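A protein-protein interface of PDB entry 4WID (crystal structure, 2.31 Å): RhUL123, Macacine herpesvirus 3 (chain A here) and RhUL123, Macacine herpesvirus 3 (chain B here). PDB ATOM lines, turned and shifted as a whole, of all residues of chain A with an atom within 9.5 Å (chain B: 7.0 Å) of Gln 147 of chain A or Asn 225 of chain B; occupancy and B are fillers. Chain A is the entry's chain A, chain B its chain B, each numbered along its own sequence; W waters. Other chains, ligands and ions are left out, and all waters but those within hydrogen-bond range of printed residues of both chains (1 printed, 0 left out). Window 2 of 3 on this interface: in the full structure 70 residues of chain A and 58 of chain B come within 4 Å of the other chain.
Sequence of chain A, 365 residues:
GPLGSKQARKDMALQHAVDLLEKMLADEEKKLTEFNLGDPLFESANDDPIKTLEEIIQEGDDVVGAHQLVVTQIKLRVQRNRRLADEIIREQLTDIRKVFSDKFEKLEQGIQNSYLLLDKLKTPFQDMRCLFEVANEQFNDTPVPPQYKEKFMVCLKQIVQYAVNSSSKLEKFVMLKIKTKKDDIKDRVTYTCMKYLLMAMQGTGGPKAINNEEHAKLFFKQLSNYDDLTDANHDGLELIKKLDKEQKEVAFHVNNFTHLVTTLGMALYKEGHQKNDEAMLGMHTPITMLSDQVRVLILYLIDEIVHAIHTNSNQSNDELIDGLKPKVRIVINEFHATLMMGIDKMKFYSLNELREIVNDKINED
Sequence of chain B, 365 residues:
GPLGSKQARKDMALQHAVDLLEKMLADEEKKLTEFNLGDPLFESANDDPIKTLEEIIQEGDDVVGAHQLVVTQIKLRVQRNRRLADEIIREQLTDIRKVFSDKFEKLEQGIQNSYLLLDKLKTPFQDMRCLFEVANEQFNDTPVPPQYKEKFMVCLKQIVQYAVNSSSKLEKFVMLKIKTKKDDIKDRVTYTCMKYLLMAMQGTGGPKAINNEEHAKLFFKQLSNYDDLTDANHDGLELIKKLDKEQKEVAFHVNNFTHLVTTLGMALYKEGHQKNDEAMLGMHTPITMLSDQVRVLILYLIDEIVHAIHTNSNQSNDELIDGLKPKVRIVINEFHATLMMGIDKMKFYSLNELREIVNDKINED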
ATOM      1  N   PRO A 143       8.465 -26.338  12.752  1.00  0.00           N
ATOM      2  CA  PRO A 143       7.324 -25.588  12.226  1.00  0.00           C
ATOM      3  C   PRO A 143       7.739 -24.788  10.996  1.00  0.00           C
ATOM      4  O   PRO A 143       8.839 -24.246  10.973  1.00  0.00           O
ATOM      5  CB  PRO A 143       6.946 -24.657  13.380  1.00  0.00           C
ATOM      6  CG  PRO A 143       8.245 -24.441  14.113  1.00  0.00           C
ATOM      7  CD  PRO A 143       9.034 -25.715  13.968  1.00  0.00           C
ATOM      8  N   VAL A 144       6.871 -24.722   9.990  1.00  0.00           N
ATOM      9  CA  VAL A 144       7.168 -24.013   8.750  1.00  0.00           C
ATOM     10  C   VAL A 144       5.845 -23.413   8.263  1.00  0.00           C
ATOM     11  O   VAL A 144       4.825 -24.093   8.269  1.00  0.00           O
ATOM     12  CB  VAL A 144       7.815 -24.962   7.707  1.00  0.00           C
ATOM     13  CG1 VAL A 144       7.639 -24.459   6.305  1.00  0.00           C
ATOM     14  CG2 VAL A 144       9.298 -25.141   8.004  1.00  0.00           C
ATOM     15  N   PRO A 145       5.840 -22.118   7.916  1.00  0.00           N
ATOM     16  CA  PRO A 145       4.581 -21.583   7.369  1.00  0.00           C
ATOM     17  C   PRO A 145       4.134 -22.482   6.228  1.00  0.00           C
ATOM     18  O   PRO A 145       4.969 -22.914   5.447  1.00  0.00           O
ATOM     19  CB  PRO A 145       4.963 -20.180   6.891  1.00  0.00           C
ATOM     20  CG  PRO A 145       6.129 -19.803   7.780  1.00  0.00           C
ATOM     21  CD  PRO A 145       6.903 -21.098   7.974  1.00  0.00           C
ATOM     22  N   PRO A 146       2.855 -22.838   6.200  1.00  0.00           N
ATOM     23  CA  PRO A 146       2.291 -23.815   5.261  1.00  0.00           C
ATOM     24  C   PRO A 146       2.744 -23.634   3.800  1.00  0.00           C
ATOM     25  O   PRO A 146       3.061 -24.635   3.138  1.00  0.00           O
ATOM     26  CB  PRO A 146       0.767 -23.588   5.392  1.00  0.00           C
ATOM     27  CG  PRO A 146       0.618 -22.220   6.031  1.00  0.00           C
ATOM     28  CD  PRO A 146       1.804 -22.143   6.961  1.00  0.00           C
ATOM     29  N   GLN A 147       2.804 -22.390   3.325  1.00  0.00           N
ATOM     30  CA  GLN A 147       3.139 -22.121   1.922  1.00  0.00           C
ATOM     31  C   GLN A 147       4.577 -22.526   1.600  1.00  0.00           C
ATOM     32  O   GLN A 147       4.983 -22.527   0.437  1.00  0.00           O
ATOM     33  CB  GLN A 147       2.928 -20.639   1.578  1.00  0.00           C
ATOM     34  CG  GLN A 147       3.947 -19.670   2.211  1.00  0.00           C
ATOM     35  CD  GLN A 147       3.421 -18.981   3.473  1.00  0.00           C
ATOM     36  OE1 GLN A 147       2.469 -19.457   4.109  1.00  0.00           O
ATOM     37  NE2 GLN A 147       4.030 -17.851   3.830  1.00  0.00           N
ATOM     38  N   TYR A 148       5.344 -22.870   2.632  1.00  0.00           N
ATOM     39  CA  TYR A 148       6.749 -23.215   2.454  1.00  0.00           C
ATOM     40  C   TYR A 148       7.057 -24.706   2.636  1.00  0.00           C
ATOM     41  O   TYR A 148       8.192 -25.129   2.384  1.00  0.00           O
ATOM     42  CB  TYR A 148       7.618 -22.408   3.429  1.00  0.00           C
ATOM     43  CG  TYR A 148       7.775 -20.952   3.057  1.00  0.00           C
ATOM     44  CD1 TYR A 148       7.544 -20.525   1.755  1.00  0.00           C
ATOM     45  CD2 TYR A 148       8.174 -20.001   4.000  1.00  0.00           C
ATOM     46  CE1 TYR A 148       7.696 -19.195   1.390  1.00  0.00           C
ATOM     47  CE2 TYR A 148       8.329 -18.659   3.643  1.00  0.00           C
ATOM     48  CZ  TYR A 148       8.082 -18.267   2.331  1.00  0.00           C
ATOM     49  OH  TYR A 148       8.215 -16.945   1.941  1.00  0.00           O
ATOM     50  N   LYS A 149       6.064 -25.489   3.063  1.00  0.00           N
ATOM     51  CA  LYS A 149       6.312 -26.846   3.575  1.00  0.00           C
ATOM     52  C   LYS A 149       6.861 -27.791   2.508  1.00  0.00           C
ATOM     53  O   LYS A 149       7.813 -28.544   2.764  1.00  0.00           O
ATOM     54  CB  LYS A 149       5.037 -27.443   4.179  1.00  0.00           C
ATOM     55  CG  LYS A 149       5.215 -28.797   4.877  1.00  0.00           C
ATOM     56  CD  LYS A 149       6.033 -28.682   6.169  1.00  0.00           C
ATOM     57  CE  LYS A 149       5.968 -29.974   7.046  1.00  0.00           C
ATOM     58  NZ  LYS A 149       6.860 -29.954   8.280  1.00  0.00           N
ATOM     59  N   GLU A 150       6.275 -27.733   1.313  1.00  0.00           N
ATOM     60  CA  GLU A 150       6.629 -28.654   0.233  1.00  0.00           C
ATOM     61  C   GLU A 150       8.039 -28.439  -0.291  1.00  0.00           C
ATOM     62  O   GLU A 150       8.773 -29.392  -0.492  1.00  0.00           O
ATOM     63  CB  GLU A 150       5.635 -28.533  -0.922  1.00  0.00           C
ATOM     64  CG  GLU A 150       5.993 -29.419  -2.100  1.00  0.00           C
ATOM     65  CD  GLU A 150       4.776 -29.946  -2.818  1.00  0.00           C
ATOM     66  OE1 GLU A 150       4.400 -29.353  -3.858  1.00  0.00           O
ATOM     67  OE2 GLU A 150       4.197 -30.952  -2.337  1.00  0.00           O
ATOM     68  N   MLY A 151       8.398 -27.181  -0.534  1.00  0.00           N
ATOM     69  CA  MLY A 151       9.755 -26.809  -0.901  1.00  0.00           C
ATOM     70  CB  MLY A 151       9.821 -25.304  -1.179  1.00  0.00           C
ATOM     71  CG  MLY A 151      11.168 -24.872  -1.721  1.00  0.00           C
ATOM     72  CD  MLY A 151      11.137 -23.535  -2.458  1.00  0.00           C
ATOM     73  CE  MLY A 151      12.576 -23.174  -2.884  1.00  0.00           C
ATOM     74  NZ  MLY A 151      12.697 -22.100  -3.921  1.00  0.00           N
ATOM     75  CH1 MLY A 151      11.645 -22.253  -4.948  1.00  0.00           C
ATOM     76  CH2 MLY A 151      12.614 -20.788  -3.266  1.00  0.00           C
ATOM     77  C   MLY A 151      10.771 -27.186   0.196  1.00  0.00           C
ATOM     78  O   MLY A 151      11.880 -27.654  -0.088  1.00  0.00           O
ATOM     79  N   PHE A 152      10.388 -26.950   1.446  1.00  0.00           N
ATOM     80  CA  PHE A 152      11.220 -27.302   2.588  1.00  0.00           C
ATOM     81  C   PHE A 152      11.541 -28.791   2.533  1.00  0.00           C
ATOM     82  O   PHE A 152      12.717 -29.197   2.570  1.00  0.00           O
ATOM     83  CB  PHE A 152      10.508 -26.924   3.897  1.00  0.00           C
ATOM     84  CG  PHE A 152      11.215 -27.409   5.148  1.00  0.00           C
ATOM     85  CD1 PHE A 152      12.590 -27.239   5.304  1.00  0.00           C
ATOM     86  CD2 PHE A 152      10.498 -28.025   6.157  1.00  0.00           C
ATOM     87  CE1 PHE A 152      13.232 -27.681   6.446  1.00  0.00           C
ATOM     88  CE2 PHE A 152      11.138 -28.479   7.314  1.00  0.00           C
ATOM     89  CZ  PHE A 152      12.505 -28.294   7.460  1.00  0.00           C
ATOM     90  N   MET A 153      10.473 -29.574   2.406  1.00  0.00           N
ATOM     91  CA  MET A 153      10.500 -31.028   2.240  1.00  0.00           C
ATOM     92  C   MET A 153      11.404 -31.489   1.089  1.00  0.00           C
ATOM     93  O   MET A 153      12.305 -32.336   1.283  1.00  0.00           O
ATOM     94  CB  MET A 153       9.063 -31.528   2.016  1.00  0.00           C
ATOM     95  CG  MET A 153       8.869 -33.053   2.059  1.00  0.00           C
ATOM     96  SD  MET A 153       9.000 -33.879   0.452  1.00  0.00           S
ATOM     97  CE  MET A 153       7.891 -32.863  -0.527  1.00  0.00           C
ATOM     98  N   VAL A 306      15.234 -23.158   5.298  1.00  0.00           N
ATOM     99  CA  VAL A 306      14.099 -22.262   5.489  1.00  0.00           C
ATOM    100  C   VAL A 306      14.525 -20.806   5.253  1.00  0.00           C
ATOM    101  O   VAL A 306      13.774 -20.044   4.649  1.00  0.00           O
ATOM    102  CB  VAL A 306      13.452 -22.403   6.898  1.00  0.00           C
ATOM    103  CG1 VAL A 306      13.067 -23.855   7.150  1.00  0.00           C
ATOM    104  CG2 VAL A 306      14.360 -21.855   7.989  1.00  0.00           C
ATOM    105  N   HIS A 307      15.739 -20.441   5.671  1.00  0.00           N
ATOM    106  CA  HIS A 307      16.222 -19.085   5.468  1.00  0.00           C
ATOM    107  C   HIS A 307      16.358 -18.749   3.970  1.00  0.00           C
ATOM    108  O   HIS A 307      16.037 -17.641   3.557  1.00  0.00           O
ATOM    109  CB  HIS A 307      17.558 -18.867   6.172  1.00  0.00           C
ATOM    110  CG  HIS A 307      18.114 -17.492   5.980  1.00  0.00           C
ATOM    111  ND1 HIS A 307      17.399 -16.351   6.281  1.00  0.00           N
ATOM    112  CD2 HIS A 307      19.308 -17.071   5.501  1.00  0.00           C
ATOM    113  CE1 HIS A 307      18.136 -15.289   6.013  1.00  0.00           C
ATOM    114  NE2 HIS A 307      19.297 -15.698   5.531  1.00  0.00           N
ATOM    115  N   ILE A 309      14.683 -20.313   1.502  1.00  0.00           N
ATOM    116  CA  ILE A 309      13.329 -20.347   0.962  1.00  0.00           C
ATOM    117  C   ILE A 309      12.647 -18.999   1.160  1.00  0.00           C
ATOM    118  O   ILE A 309      12.017 -18.459   0.252  1.00  0.00           O
ATOM    119  CB  ILE A 309      12.472 -21.443   1.631  1.00  0.00           C
ATOM    120  CG1 ILE A 309      12.892 -22.831   1.161  1.00  0.00           C
ATOM    121  CG2 ILE A 309      10.998 -21.240   1.326  1.00  0.00           C
ATOM    122  CD1 ILE A 309      12.217 -23.936   1.903  1.00  0.00           C
ATOM    123  N   HIS A 310      12.786 -18.473   2.367  1.00  0.00           N
ATOM    124  CA  HIS A 310      12.245 -17.179   2.717  1.00  0.00           C
ATOM    125  C   HIS A 310      12.821 -16.047   1.848  1.00  0.00           C
ATOM    126  O   HIS A 310      12.095 -15.302   1.192  1.00  0.00           O
ATOM    127  CB  HIS A 310      12.534 -16.920   4.190  1.00  0.00           C
ATOM    128  CG  HIS A 310      11.961 -15.641   4.706  1.00  0.00           C
ATOM    129  ND1 HIS A 310      12.442 -15.014   5.841  1.00  0.00           N
ATOM    130  CD2 HIS A 310      10.930 -14.884   4.265  1.00  0.00           C
ATOM    131  CE1 HIS A 310      11.748 -13.911   6.058  1.00  0.00           C
ATOM    132  NE2 HIS A 310      10.824 -13.808   5.116  1.00  0.00           N
ATOM    133  N   THR A 311      14.141 -15.988   1.833  1.00  0.00           N
ATOM    134  CA  THR A 311      14.952 -14.862   1.402  1.00  0.00           C
ATOM    135  C   THR A 311      15.322 -14.886  -0.102  1.00  0.00           C
ATOM    136  O   THR A 311      15.835 -13.908  -0.662  1.00  0.00           O
ATOM    137  CB  THR A 311      16.210 -14.856   2.321  1.00  0.00           C
ATOM    138  OG1 THR A 311      15.871 -14.208   3.554  1.00  0.00           O
ATOM    139  CG2 THR A 311      17.437 -14.217   1.714  1.00  0.00           C
ATOM    140  N   SER A 313      13.179 -16.641  -2.968  1.00  0.00           N
ATOM    141  CA  SER A 313      12.147 -17.417  -3.667  1.00  0.00           C
ATOM    142  C   SER A 313      12.341 -17.544  -5.195  1.00  0.00           C
ATOM    143  O   SER A 313      11.680 -18.367  -5.842  1.00  0.00           O
ATOM    144  CB  SER A 313      10.764 -16.822  -3.385  1.00  0.00           C
ATOM    145  OG  SER A 313      10.868 -15.479  -2.959  1.00  0.00           O
ATOM    146  N   LYS B 221      11.406 -16.713  13.745  1.00  0.00           N
ATOM    147  CA  LYS B 221      12.056 -16.188  12.557  1.00  0.00           C
ATOM    148  C   LYS B 221      10.994 -16.040  11.459  1.00  0.00           C
ATOM    149  O   LYS B 221      10.998 -15.098  10.694  1.00  0.00           O
ATOM    150  CB  LYS B 221      13.187 -17.136  12.126  1.00  0.00           C
ATOM    151  CG  LYS B 221      14.359 -16.538  11.352  1.00  0.00           C
ATOM    152  CD  LYS B 221      15.593 -17.422  11.568  1.00  0.00           C
ATOM    153  CE  LYS B 221      16.707 -17.192  10.558  1.00  0.00           C
ATOM    154  NZ  LYS B 221      17.910 -17.989  10.954  1.00  0.00           N
ATOM    155  N   GLN B 222      10.057 -16.974  11.443  1.00  0.00           N
ATOM    156  CA  GLN B 222       9.089 -17.095  10.378  1.00  0.00           C
ATOM    157  C   GLN B 222       7.679 -16.641  10.789  1.00  0.00           C
ATOM    158  O   GLN B 222       6.738 -16.757   9.990  1.00  0.00           O
ATOM    159  CB  GLN B 222       9.049 -18.551   9.891  1.00  0.00           C
ATOM    160  CG  GLN B 222      10.260 -18.985   9.057  1.00  0.00           C
ATOM    161  CD  GLN B 222      10.376 -18.190   7.739  1.00  0.00           C
ATOM    162  OE1 GLN B 222       9.371 -17.896   7.085  1.00  0.00           O
ATOM    163  NE2 GLN B 222      11.608 -17.834   7.357  1.00  0.00           N
ATOM    164  N   LEU B 223       7.524 -16.112  12.001  1.00  0.00           N
ATOM    165  CA  LEU B 223       6.176 -15.792  12.505  1.00  0.00           C
ATOM    166  C   LEU B 223       5.443 -14.800  11.607  1.00  0.00           C
ATOM    167  O   LEU B 223       4.231 -14.860  11.484  1.00  0.00           O
ATOM    168  CB  LEU B 223       6.215 -15.225  13.925  1.00  0.00           C
ATOM    169  CG  LEU B 223       5.584 -16.045  15.060  1.00  0.00           C
ATOM    170  CD1 LEU B 223       5.593 -15.245  16.370  1.00  0.00           C
ATOM    171  CD2 LEU B 223       4.193 -16.527  14.736  1.00  0.00           C
ATOM    172  N   SER B 224       6.178 -13.879  10.999  1.00  0.00           N
ATOM    173  CA  SER B 224       5.534 -12.869  10.170  1.00  0.00           C
ATOM    174  C   SER B 224       5.077 -13.415   8.807  1.00  0.00           C
ATOM    175  O   SER B 224       4.293 -12.781   8.100  1.00  0.00           O
ATOM    176  CB  SER B 224       6.462 -11.677   9.979  1.00  0.00           C
ATOM    177  OG  SER B 224       6.151 -10.683  10.933  1.00  0.00           O
ATOM    178  N   ASN B 225       5.539 -14.606   8.458  1.00  0.00           N
ATOM    179  CA  ASN B 225       5.134 -15.220   7.210  1.00  0.00           C
ATOM    180  C   ASN B 225       3.974 -16.165   7.349  1.00  0.00           C
ATOM    181  O   ASN B 225       3.627 -16.853   6.398  1.00  0.00           O
ATOM    182  CB  ASN B 225       6.294 -15.981   6.594  1.00  0.00           C
ATOM    183  CG  ASN B 225       7.447 -15.105   6.318  1.00  0.00           C
ATOM    184  OD1 ASN B 225       7.278 -13.927   5.988  1.00  0.00           O
ATOM    185  ND2 ASN B 225       8.646 -15.653   6.464  1.00  0.00           N
ATOM    186  N   TYR B 226       3.394 -16.248   8.534  1.00  0.00           N
ATOM    187  CA  TYR B 226       2.168 -17.007   8.659  1.00  0.00           C
ATOM    188  C   TYR B 226       1.029 -16.081   8.222  1.00  0.00           C
ATOM    189  O   TYR B 226       0.790 -15.059   8.862  1.00  0.00           O
ATOM    190  CB  TYR B 226       1.949 -17.505  10.091  1.00  0.00           C
ATOM    191  CG  TYR B 226       2.739 -18.750  10.492  1.00  0.00           C
ATOM    192  CD1 TYR B 226       2.192 -20.025  10.339  1.00  0.00           C
ATOM    193  CD2 TYR B 226       4.017 -18.650  11.061  1.00  0.00           C
ATOM    194  CE1 TYR B 226       2.887 -21.149  10.717  1.00  0.00           C
ATOM    195  CE2 TYR B 226       4.719 -19.778  11.449  1.00  0.00           C
ATOM    196  CZ  TYR B 226       4.149 -21.027  11.278  1.00  0.00           C
ATOM    197  OH  TYR B 226       4.827 -22.164  11.663  1.00  0.00           O
ATOM    198  N   ASP B 227       0.339 -16.431   7.139  1.00  0.00           N
ATOM    199  CA  ASP B 227      -0.783 -15.609   6.659  1.00  0.00           C
ATOM    200  C   ASP B 227      -1.921 -15.694   7.650  1.00  0.00           C
ATOM    201  O   ASP B 227      -2.657 -14.721   7.898  1.00  0.00           O
ATOM    202  CB  ASP B 227      -1.269 -16.062   5.277  1.00  0.00           C
ATOM    203  CG  ASP B 227      -0.353 -15.619   4.165  1.00  0.00           C
ATOM    204  OD1 ASP B 227       0.573 -14.822   4.436  1.00  0.00           O
ATOM    205  OD2 ASP B 227      -0.574 -16.050   3.009  1.00  0.00           O
ATOM    206  N   ASP B 228      -2.050 -16.880   8.225  1.00  0.00           N
ATOM    207  CA  ASP B 228      -3.203 -17.187   9.045  1.00  0.00           C
ATOM    208  C   ASP B 228      -2.716 -17.561  10.452  1.00  0.00           C
ATOM    209  O   ASP B 228      -1.985 -18.548  10.630  1.00  0.00           O
ATOM    210  CB  ASP B 228      -4.006 -18.296   8.368  1.00  0.00           C
ATOM    211  CG  ASP B 228      -5.163 -18.800   9.200  1.00  0.00           C
ATOM    212  OD1 ASP B 228      -5.520 -18.172  10.227  1.00  0.00           O
ATOM    213  OD2 ASP B 228      -5.721 -19.850   8.802  1.00  0.00           O
ATOM    214  N   ASP B 231      -2.711 -21.127  12.004  1.00  0.00           N
ATOM    215  CA  ASP B 231      -1.583 -21.970  11.631  1.00  0.00           C
ATOM    216  C   ASP B 231      -0.448 -21.769  12.609  1.00  0.00           C
ATOM    217  O   ASP B 231       0.107 -22.732  13.130  1.00  0.00           O
ATOM    218  CB  ASP B 231      -1.089 -21.654  10.219  1.00  0.00           C
ATOM    219  CG  ASP B 231      -2.074 -22.083   9.143  1.00  0.00           C
ATOM    220  OD1 ASP B 231      -2.955 -22.909   9.450  1.00  0.00           O
ATOM    221  OD2 ASP B 231      -1.960 -21.602   7.994  1.00  0.00           O
HETATM  222  O   HOH W   1       0.658 -18.594   5.632  1.00  0.00           O
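The side-chain amide nitrogen (ND2) of Asn 225 of chain B sits at hydrogen-bond distance from a ring nitrogen (NE2) of His 310 of chain A. ND1 of His 310 of chain A lies within hydrogen-bond range of NE2 of Gln 222 of chain B, 3.3 Å away. The side-chain amide nitrogen (NE2) of Gln 147 of chain A sits at hydrogen-bond distance from the backbone carbonyl oxygen (O) of Asn 225 of chain B (2.8 Å).
The side-chain amide oxygen (OE1) of Gln 222 of chain B sits at hydrogen-bond distance from the side-chain amide nitrogen (ND2) of Asn 225 of chain B, at 2.4 Å.
Pro 143 of chain A touches Tyr 226 of chain B. N of Val 144 of chain A touches OH of Tyr 226 of chain B, at 3.7 Å. Pro 145 of chain A touches Gln 222 of chain B. Pro 145 of chain A touches Asn 225 of chain B (CB to O, 3.6 Å). Pro 145 of chain A touches Tyr 226 of chain B (CA to CE1, 3.8 Å). Asp 231 of chain B touches Pro 146 of chain A (OD2 to CG, 3.3 Å). CE2 of Tyr 148 of chain A touches OE1 of Gln 222 of chain B, at 3.7 Å.
Of the printed residues of chain B, Pro 145 of chain A touches Gln 222, Asn 225 and Tyr 226. Of the printed residues of chain B, Pro 146 of chain A touches Asp 231. Gln 147 of chain A touches just one residue of chain B: Asn 225 (2.8 Å). His 307 of chain A touches none of the printed residues of chain B. Gln 222 of chain B touches just these residues of chain A: Pro 145 (3.8 Å), Tyr 148 (3.7 Å) and His 310 (3.3 Å). No residue of chain A comes within 4 Å of Ser 224 of chain B. Asn 225 of chain B touches three residues of chain A. Of the printed residues of chain A, Tyr 226 of chain B touches Pro 143, Val 144 and Pro 145. Asp 228 of chain B touches none of the printed residues of chain A. The nearest residue of chain B that does not touch Gln 147 of chain A is Asp 227 of chain B (4.6 Å). The nearest residue of chain A that does not touch Asn 225 of chain B is Tyr 148 of chain A (4.1 Å).
Of the 17 printed residues of chain A, 7 touch a printed residue of chain B. Printed residues of chain A that touch a printed residue of chain B: Pro 143, Val 144, Pro 145, Pro 146, Gln 147, Tyr 148 and His 310. Hydrophobic or aromatic side chains of chain A that line the printed part of chain B: Pro 143, Pro 145, Pro 146, Tyr 148 and His 310. Along chain A the printed residues that touch a printed residue of chain B span positions 143 to 310. Printed residues of chain B that touch a printed residue of chain A: Gln 222, Asn 225, Tyr 226 and Asp 231. Hydrophobic or aromatic side chains of chain B that line the printed part of chain A: Tyr 226. Along chain B the printed residues that touch a printed residue of chain A span positions 222 to 231. Among the printed residues, 10 pairs touch across the chains. Among the printed residues, no Asp or Glu carboxylate lies within 4 Å of a Lys or Arg side-chain nitrogen of the other chain.
Water W1 lies within hydrogen-bond range of OE1 of Gln 147 of chain A (2.5 Å) and N of Asp 227 of chain B (2.7 Å).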
